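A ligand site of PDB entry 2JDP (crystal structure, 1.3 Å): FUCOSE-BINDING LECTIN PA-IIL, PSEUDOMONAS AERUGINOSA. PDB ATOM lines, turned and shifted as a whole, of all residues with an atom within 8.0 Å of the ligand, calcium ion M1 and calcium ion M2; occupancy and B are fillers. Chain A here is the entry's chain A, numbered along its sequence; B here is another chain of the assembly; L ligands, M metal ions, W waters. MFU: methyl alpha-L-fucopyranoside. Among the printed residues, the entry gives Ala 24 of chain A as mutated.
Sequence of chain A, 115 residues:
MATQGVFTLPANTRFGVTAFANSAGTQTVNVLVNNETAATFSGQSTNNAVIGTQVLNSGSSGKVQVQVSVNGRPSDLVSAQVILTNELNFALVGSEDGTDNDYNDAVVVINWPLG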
ATOM      1  N   ALA A  21      14.083  15.589  14.955  1.00  0.00           N
ATOM      2  CA  ALA A  21      12.835  16.329  14.610  1.00  0.00           C
ATOM      3  C   ALA A  21      11.636  15.848  15.420  1.00  0.00           C
ATOM      4  O   ALA A  21      11.481  14.661  15.696  1.00  0.00           O
ATOM      5  CB  ALA A  21      12.571  16.222  13.080  1.00  0.00           C
ATOM      6  N   ASN A  22      10.804  16.832  15.809  1.00  0.00           N
ATOM      7  CA  ASN A  22       9.575  16.586  16.577  1.00  0.00           C
ATOM      8  C   ASN A  22       8.556  17.631  16.178  1.00  0.00           C
ATOM      9  O   ASN A  22       8.203  18.543  16.943  1.00  0.00           O
ATOM     10  CB  ASN A  22       9.833  16.714  18.071  1.00  0.00           C
ATOM     11  CG  ASN A  22      10.701  15.606  18.618  1.00  0.00           C
ATOM     12  OD1 ASN A  22      10.247  14.470  18.839  1.00  0.00           O
ATOM     13  ND2 ASN A  22      11.978  15.940  18.891  1.00  0.00           N
ATOM     14  N   SER A  23       8.100  17.551  14.946  1.00  0.00           N
ATOM     15  CA  SER A  23       7.132  18.541  14.417  1.00  0.00           C
ATOM     16  C   SER A  23       6.389  17.925  13.262  1.00  0.00           C
ATOM     17  O   SER A  23       6.912  17.027  12.582  1.00  0.00           O
ATOM     18  CB  SER A  23       7.879  19.793  13.924  1.00  0.00           C
ATOM     19  OG  SER A  23       7.021  20.692  13.185  1.00  0.00           O
ATOM     20  N   ALA A  24       5.175  18.412  13.012  1.00  0.00           N
ATOM     21  CA  ALA A  24       4.461  18.055  11.775  1.00  0.00           C
ATOM     22  C   ALA A  24       5.161  18.587  10.532  1.00  0.00           C
ATOM     23  O   ALA A  24       4.973  18.057   9.431  1.00  0.00           O
ATOM     24  CB  ALA A  24       3.018  18.573  11.816  1.00  0.00           C
ATOM     25  N   GLY A  25       5.944  19.657  10.684  1.00  0.00           N
ATOM     26  CA  GLY A  25       6.623  20.299   9.581  1.00  0.00           C
ATOM     27  C   GLY A  25       8.021  19.768   9.329  1.00  0.00           C
ATOM     28  O   GLY A  25       8.710  19.342  10.248  1.00  0.00           O
ATOM     29  N   GLN A  27      11.774  19.977   8.981  1.00  0.00           N
ATOM     30  CA  GLN A  27      12.806  20.837   9.561  1.00  0.00           C
ATOM     31  C   GLN A  27      14.031  20.883   8.681  1.00  0.00           C
ATOM     32  O   GLN A  27      14.475  19.827   8.192  1.00  0.00           O
ATOM     33  CB  GLN A  27      13.215  20.278  10.931  1.00  0.00           C
ATOM     34  CG  GLN A  27      12.039  20.071  11.858  1.00  0.00           C
ATOM     35  CD  GLN A  27      11.380  21.382  12.277  1.00  0.00           C
ATOM     36  OE1 GLN A  27      12.061  22.306  12.744  1.00  0.00           O
ATOM     37  NE2 GLN A  27      10.048  21.475  12.107  1.00  0.00           N
ATOM     38  N   GLN A  44      11.460  15.043   8.528  1.00  0.00           N
ATOM     39  CA  GLN A  44      10.227  15.236   9.279  1.00  0.00           C
ATOM     40  C   GLN A  44       9.954  14.047  10.165  1.00  0.00           C
ATOM     41  O   GLN A  44       9.966  12.887   9.707  1.00  0.00           O
ATOM     42  CB  GLN A  44       9.041  15.528   8.336  1.00  0.00           C
ATOM     43  CG  GLN A  44       7.725  15.894   9.038  1.00  0.00           C
ATOM     44  CD  GLN A  44       6.947  14.701   9.574  1.00  0.00           C
ATOM     45  OE1 GLN A  44       6.843  13.661   8.903  1.00  0.00           O
ATOM     46  NE2 GLN A  44       6.402  14.828  10.773  1.00  0.00           N
ATOM     47  N   SER A  45       9.714  14.291  11.456  1.00  0.00           N
ATOM     48  CA  SER A  45       9.344  13.249  12.376  1.00  0.00           C
ATOM     49  C   SER A  45       8.592  13.899  13.532  1.00  0.00           C
ATOM     50  O   SER A  45       8.883  15.062  13.897  1.00  0.00           O
ATOM     51  CB  SER A  45      10.620  12.573  12.937  1.00  0.00           C
ATOM     52  OG  SER A  45      10.323  11.495  13.808  1.00  0.00           O
ATOM     53  N   THR A  46       7.657  13.159  14.122  1.00  0.00           N
ATOM     54  CA  THR A  46       7.081  13.525  15.427  1.00  0.00           C
ATOM     55  C   THR A  46       7.540  12.556  16.534  1.00  0.00           C
ATOM     56  O   THR A  46       6.958  12.508  17.641  1.00  0.00           O
ATOM     57  CB  THR A  46       5.535  13.597  15.348  1.00  0.00           C
ATOM     58  OG1 THR A  46       5.040  12.403  14.730  1.00  0.00           O
ATOM     59  CG2 THR A  46       5.105  14.808  14.502  1.00  0.00           C
ATOM     60  N   VAL A  70      11.653  26.281   8.690  1.00  0.00           N
ATOM     61  CA  VAL A  70      10.515  25.408   8.402  1.00  0.00           C
ATOM     62  C   VAL A  70       9.622  26.202   7.460  1.00  0.00           C
ATOM     63  O   VAL A  70       9.292  27.350   7.748  1.00  0.00           O
ATOM     64  CB  VAL A  70       9.711  25.046   9.684  1.00  0.00           C
ATOM     65  CG1 VAL A  70       8.542  24.078   9.371  1.00  0.00           C
ATOM     66  CG2 VAL A  70      10.617  24.437  10.736  1.00  0.00           C
ATOM     67  N   ASN A  71       9.228  25.599   6.342  1.00  0.00           N
ATOM     68  CA  ASN A  71       8.356  26.259   5.349  1.00  0.00           C
ATOM     69  C   ASN A  71       8.860  27.646   4.938  1.00  0.00           C
ATOM     70  O   ASN A  71       8.074  28.616   4.860  1.00  0.00           O
ATOM     71  CB  ASN A  71       6.917  26.347   5.875  1.00  0.00           C
ATOM     72  CG  ASN A  71       6.308  24.987   6.171  1.00  0.00           C
ATOM     73  OD1 ASN A  71       5.433  24.862   7.036  1.00  0.00           O
ATOM     74  ND2 ASN A  71       6.788  23.951   5.467  1.00  0.00           N
ATOM     75  N   SER A  95      14.309  24.590  18.922  1.00  0.00           N
ATOM     76  CA  SER A  95      13.727  25.530  17.972  1.00  0.00           C
ATOM     77  C   SER A  95      12.221  25.389  17.973  1.00  0.00           C
ATOM     78  O   SER A  95      11.689  24.321  18.228  1.00  0.00           O
ATOM     79  CB  SER A  95      14.298  25.309  16.576  1.00  0.00           C
ATOM     80  OG  SER A  95      13.880  24.054  16.088  1.00  0.00           O
ATOM     81  N   GLU A  96      11.567  26.539  17.695  1.00  0.00           N
ATOM     82  CA  GLU A  96      10.122  26.601  17.678  1.00  0.00           C
ATOM     83  C   GLU A  96       9.636  27.173  16.355  1.00  0.00           C
ATOM     84  O   GLU A  96      10.041  28.264  15.941  1.00  0.00           O
ATOM     85  CB  GLU A  96       9.626  27.456  18.841  1.00  0.00           C
ATOM     86  CG  GLU A  96       8.095  27.571  18.956  1.00  0.00           C
ATOM     87  CD  GLU A  96       7.439  26.225  18.969  1.00  0.00           C
ATOM     88  OE1 GLU A  96       7.850  25.373  19.801  1.00  0.00           O
ATOM     89  OE2 GLU A  96       6.505  26.039  18.132  1.00  0.00           O
ATOM     90  N   ASP A  97       8.813  26.381  15.668  1.00  0.00           N
ATOM     91  CA  ASP A  97       8.330  26.783  14.328  1.00  0.00           C
ATOM     92  C   ASP A  97       6.890  27.283  14.355  1.00  0.00           C
ATOM     93  O   ASP A  97       6.398  27.782  13.327  1.00  0.00           O
ATOM     94  CB  ASP A  97       8.511  25.653  13.309  1.00  0.00           C
ATOM     95  CG  ASP A  97       7.698  24.408  13.654  1.00  0.00           C
ATOM     96  OD1 ASP A  97       6.590  24.537  14.245  1.00  0.00           O
ATOM     97  OD2 ASP A  97       8.121  23.297  13.281  1.00  0.00           O
ATOM     98  N   GLY A  98       6.213  27.135  15.490  1.00  0.00           N
ATOM     99  CA  GLY A  98       4.758  27.288  15.529  1.00  0.00           C
ATOM    100  C   GLY A  98       4.209  27.981  16.762  1.00  0.00           C
ATOM    101  O   GLY A  98       4.696  29.055  17.166  1.00  0.00           O
ATOM    102  N   THR A  99       3.176  27.376  17.364  1.00  0.00           N
ATOM    103  CA  THR A  99       2.387  28.066  18.381  1.00  0.00           C
ATOM    104  C   THR A  99       2.537  27.503  19.795  1.00  0.00           C
ATOM    105  O   THR A  99       2.314  28.225  20.784  1.00  0.00           O
ATOM    106  CB  THR A  99       0.869  28.141  18.013  1.00  0.00           C
ATOM    107  OG1 THR A  99       0.249  26.874  18.276  1.00  0.00           O
ATOM    108  CG2 THR A  99       0.670  28.537  16.545  1.00  0.00           C
ATOM    109  N   ASP A 100       2.899  26.227  19.902  1.00  0.00           N
ATOM    110  CA  ASP A 100       2.813  25.528  21.190  1.00  0.00           C
ATOM    111  C   ASP A 100       3.981  25.722  22.169  1.00  0.00           C
ATOM    112  O   ASP A 100       3.858  25.421  23.360  1.00  0.00           O
ATOM    113  CB  ASP A 100       2.528  24.030  20.980  1.00  0.00           C
ATOM    114  CG  ASP A 100       3.694  23.291  20.338  1.00  0.00           C
ATOM    115  OD1 ASP A 100       4.599  23.949  19.743  1.00  0.00           O
ATOM    116  OD2 ASP A 100       3.676  22.049  20.429  1.00  0.00           O
ATOM    117  N   ASN A 101       5.112  26.222  21.655  1.00  0.00           N
ATOM    118  CA  ASN A 101       6.292  26.547  22.471  1.00  0.00           C
ATOM    119  C   ASN A 101       6.950  25.375  23.207  1.00  0.00           C
ATOM    120  O   ASN A 101       7.381  25.504  24.366  1.00  0.00           O
ATOM    121  CB  ASN A 101       5.995  27.710  23.439  1.00  0.00           C
ATOM    122  CG  ASN A 101       5.617  28.985  22.706  1.00  0.00           C
ATOM    123  OD1 ASN A 101       6.182  29.302  21.640  1.00  0.00           O
ATOM    124  ND2 ASN A 101       4.651  29.728  23.254  1.00  0.00           N
ATOM    125  N   ASP A 102       7.043  24.231  22.536  1.00  0.00           N
ATOM    126  CA  ASP A 102       7.769  23.106  23.140  1.00  0.00           C
ATOM    127  C   ASP A 102       9.307  23.244  22.923  1.00  0.00           C
ATOM    128  O   ASP A 102      10.139  22.651  23.641  1.00  0.00           O
ATOM    129  CB  ASP A 102       7.159  21.722  22.774  1.00  0.00           C
ATOM    130  CG  ASP A 102       6.988  21.476  21.245  1.00  0.00           C
ATOM    131  OD1 ASP A 102       7.403  22.289  20.392  1.00  0.00           O
ATOM    132  OD2 ASP A 102       6.473  20.369  20.898  1.00  0.00           O
ATOM    133  N   TYR A 103       9.648  24.103  21.968  1.00  0.00           N
ATOM    134  CA  TYR A 103      11.030  24.315  21.471  1.00  0.00           C
ATOM    135  C   TYR A 103      11.750  23.003  21.102  1.00  0.00           C
ATOM    136  O   TYR A 103      12.970  22.897  21.171  1.00  0.00           O
ATOM    137  CB  TYR A 103      11.861  25.216  22.416  1.00  0.00           C
ATOM    138  CG  TYR A 103      11.543  26.652  22.137  1.00  0.00           C
ATOM    139  CD1 TYR A 103      12.354  27.420  21.310  1.00  0.00           C
ATOM    140  CD2 TYR A 103      10.373  27.229  22.641  1.00  0.00           C
ATOM    141  CE1 TYR A 103      12.048  28.750  21.003  1.00  0.00           C
ATOM    142  CE2 TYR A 103      10.027  28.541  22.327  1.00  0.00           C
ATOM    143  CZ  TYR A 103      10.868  29.303  21.534  1.00  0.00           C
ATOM    144  OH  TYR A 103      10.515  30.625  21.205  1.00  0.00           O
ATOM    145  N   ASN A 104      10.978  21.999  20.687  1.00  0.00           N
ATOM    146  CA  ASN A 104      11.551  20.691  20.340  1.00  0.00           C
ATOM    147  C   ASN A 104      11.385  20.374  18.851  1.00  0.00           C
ATOM    148  O   ASN A 104      11.683  19.246  18.435  1.00  0.00           O
ATOM    149  CB  ASN A 104      10.947  19.550  21.197  1.00  0.00           C
ATOM    150  CG  ASN A 104       9.537  19.195  20.762  1.00  0.00           C
ATOM    151  OD1 ASN A 104       8.983  19.827  19.858  1.00  0.00           O
ATOM    152  ND2 ASN A 104       8.963  18.183  21.381  1.00  0.00           N
ATOM    153  N   ASP A 105      10.939  21.343  18.067  1.00  0.00           N
ATOM    154  CA  ASP A 105      10.579  21.066  16.675  1.00  0.00           C
ATOM    155  C   ASP A 105      11.762  20.541  15.912  1.00  0.00           C
ATOM    156  O   ASP A 105      11.631  19.539  15.187  1.00  0.00           O
ATOM    157  CB  ASP A 105       9.957  22.313  16.041  1.00  0.00           C
ATOM    158  CG  ASP A 105       8.626  22.649  16.677  1.00  0.00           C
ATOM    159  OD1 ASP A 105       7.911  21.730  17.126  1.00  0.00           O
ATOM    160  OD2 ASP A 105       8.296  23.857  16.809  1.00  0.00           O
ATOM    161  N   ALA A 106      12.916  21.196  16.064  1.00  0.00           N
ATOM    162  CA  ALA A 106      14.210  20.617  15.749  1.00  0.00           C
ATOM    163  C   ALA A 106      15.058  20.761  17.007  1.00  0.00           C
ATOM    164  O   ALA A 106      15.120  21.875  17.568  1.00  0.00           O
ATOM    165  CB  ALA A 106      14.875  21.342  14.633  1.00  0.00           C
ATOM    166  N   VAL A 107      15.711  19.679  17.426  1.00  0.00           N
ATOM    167  CA  VAL A 107      16.614  19.675  18.592  1.00  0.00           C
ATOM    168  C   VAL A 107      18.005  19.378  18.021  1.00  0.00           C
ATOM    169  O   VAL A 107      18.151  18.419  17.257  1.00  0.00           O
ATOM    170  CB  VAL A 107      16.191  18.610  19.587  1.00  0.00           C
ATOM    171  CG1 VAL A 107      17.241  18.449  20.728  1.00  0.00           C
ATOM    172  CG2 VAL A 107      14.795  18.930  20.229  1.00  0.00           C
ATOM    173  N   PRO B 113      10.474  17.111  26.016  1.00  0.00           N
ATOM    174  CA  PRO B 113       9.441  16.203  25.481  1.00  0.00           C
ATOM    175  C   PRO B 113       9.666  15.964  23.990  1.00  0.00           C
ATOM    176  O   PRO B 113      10.387  16.704  23.318  1.00  0.00           O
ATOM    177  CB  PRO B 113       8.141  16.981  25.716  1.00  0.00           C
ATOM    178  CG  PRO B 113       8.541  18.403  25.618  1.00  0.00           C
ATOM    179  CD  PRO B 113       9.974  18.486  26.192  1.00  0.00           C
ATOM    180  N   LEU B 114       9.016  14.916  23.511  1.00  0.00           N
ATOM    181  CA  LEU B 114       8.992  14.631  22.069  1.00  0.00           C
ATOM    182  C   LEU B 114       7.669  15.095  21.447  1.00  0.00           C
ATOM    183  O   LEU B 114       6.750  15.580  22.158  1.00  0.00           O
ATOM    184  CB  LEU B 114       9.199  13.133  21.805  1.00  0.00           C
ATOM    185  CG  LEU B 114      10.377  12.493  22.518  1.00  0.00           C
ATOM    186  CD1 LEU B 114      10.534  11.029  22.091  1.00  0.00           C
ATOM    187  CD2 LEU B 114      11.654  13.276  22.266  1.00  0.00           C
ATOM    188  N   GLY B 115       7.528  14.885  20.140  1.00  0.00           N
ATOM    189  CA  GLY B 115       6.245  15.137  19.467  1.00  0.00           C
ATOM    190  C   GLY B 115       6.060  16.534  18.911  1.00  0.00           C
ATOM    191  O   GLY B 115       6.670  17.514  19.387  1.00  0.00           O
ATOM    192  OXT GLY B 115       5.322  16.689  17.930  1.00  0.00           O
HETATM  193  C1  MFU L   1       4.077  21.501  14.783  1.00  0.00           C
HETATM  194  C2  MFU L   1       4.956  21.749  15.981  1.00  0.00           C
HETATM  195  C3  MFU L   1       4.266  21.203  17.223  1.00  0.00           C
HETATM  196  C4  MFU L   1       3.919  19.723  17.109  1.00  0.00           C
HETATM  197  C5  MFU L   1       3.160  19.470  15.796  1.00  0.00           C
HETATM  198  C6  MFU L   1       2.891  17.985  15.509  1.00  0.00           C
HETATM  199  O1  MFU L   1       2.853  22.252  14.909  1.00  0.00           O
HETATM  200  O2  MFU L   1       5.132  23.156  16.167  1.00  0.00           O
HETATM  201  O3  MFU L   1       5.140  21.408  18.353  1.00  0.00           O
HETATM  202  O4  MFU L   1       5.154  18.985  17.172  1.00  0.00           O
HETATM  203  O5  MFU L   1       3.841  20.084  14.700  1.00  0.00           O
HETATM  204  CM  MFU L   1       2.151  22.309  13.669  1.00  0.00           C
HETATM  205 CA    CA M   1       7.080  19.820  18.499  1.00  0.00          CA
HETATM  206 CA    CA M   2       6.510  23.495  18.398  1.00  0.00          CA
HETATM  207  O   HOH W   1       1.547  14.908  15.607  1.00  0.00           O
HETATM  208  O   HOH W   2       2.856  24.486  16.871  1.00  0.00           O
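Within 4 Å of calcium ion M2: Glu 96, Asp 100, Asp 102 and Asp 105. The nearest printed residue that does not touch calcium ion M2 is Asp 97 (4.3 Å).
Calcium ion M1 is bound by the backbone carbonyl oxygen (O) of Asn 22 (2.3 Å), the side-chain amide oxygen (OD1) of Asn 104 (2.3 Å), an oxygen (O4) of the ligand (2.5 Å), the side-chain carboxylate (OD1) of Asp 105 (2.5 Å), the chain-end carboxylate (O) of Gly 115 of chain B (2.5 Å), an oxygen (O3) of the ligand (2.5 Å) and the side-chain carboxylate (OD2) of Asp 102 (2.5 Å). Calcium ion M1 has seven donor atoms within binding distance. Slightly farther from calcium ion M1 lies the side-chain carboxylate (OD1) of Asp 102 (3.1 Å).
Within 4 Å of calcium ion M1: Asn 22, Asp 102, Asn 104, Asp 105 and Gly 115 of chain B. The nearest printed residue that does not touch calcium ion M1 is Ser 23 (4.3 Å).
The side-chain carboxylate (OD1) of Asp 100 binds calcium ion M2 (2.4 Å). Calcium ion M2 is bound by the side-chain carboxylate (OD2) of Asp 105, at 2.4 Å. Calcium ion M2 is bound by the side-chain carboxylate (OD1) of Asp 102. Calcium ion M2 is bound by O3 of the ligand (2.5 Å). OE2 of Glu 96 binds calcium ion M2 (2.6 Å). OD1 of Asp 105 binds calcium ion M2 (2.6 Å). O2 of the ligand is bound to calcium ion M2 (2.6 Å). OE1 of Glu 96 binds calcium ion M2 (2.7 Å).
O2 of the ligand sits close to OD1 of Asp 97. O5 of the ligand lies within hydrogen-bond range of N of Ala 24 (2.7 Å).
The backbone NH (N) of Asn 101 lies close to the side-chain carboxylate (OE1) of Glu 96 (3.4 Å). NE2 of Gln 27 sits at hydrogen-bond distance from OD2 of Asp 97, at 2.9 Å. The side-chain carboxylate (OE1) of Glu 96 lies close to the backbone NH (N) of Tyr 103 (3.1 Å). OE2 of Glu 96 lies close to N of Gly 98, at 2.9 Å. NE2 of Gln 44 sits at hydrogen-bond distance from O of Ser 23 (2.9 Å). The side-chain hydroxyl of Ser 23 sits at hydrogen-bond distance from the backbone NH of Gly 25 (2.9 Å). OD2 of Asp 97 lies within hydrogen-bond range of OG of Ser 23 (2.8 Å). The side-chain amide nitrogen (ND2) of Asn 104 sits at hydrogen-bond distance from the backbone carbonyl oxygen (O) of Pro 113 of chain B (2.8 Å).
Ser 23 touches the ligand (CA to O4, 3.4 Å). Hydrophobic or aromatic side chains within 4 Å of the ligand: Ala 24. Of the 27 residues printed, 9 come within 4 Å of the ligand.
Water W2 lies within hydrogen-bond range of N of Thr 99 (2.9 Å), O1 of the ligand (3.0 Å) and N of Asp 100 (3.5 Å).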
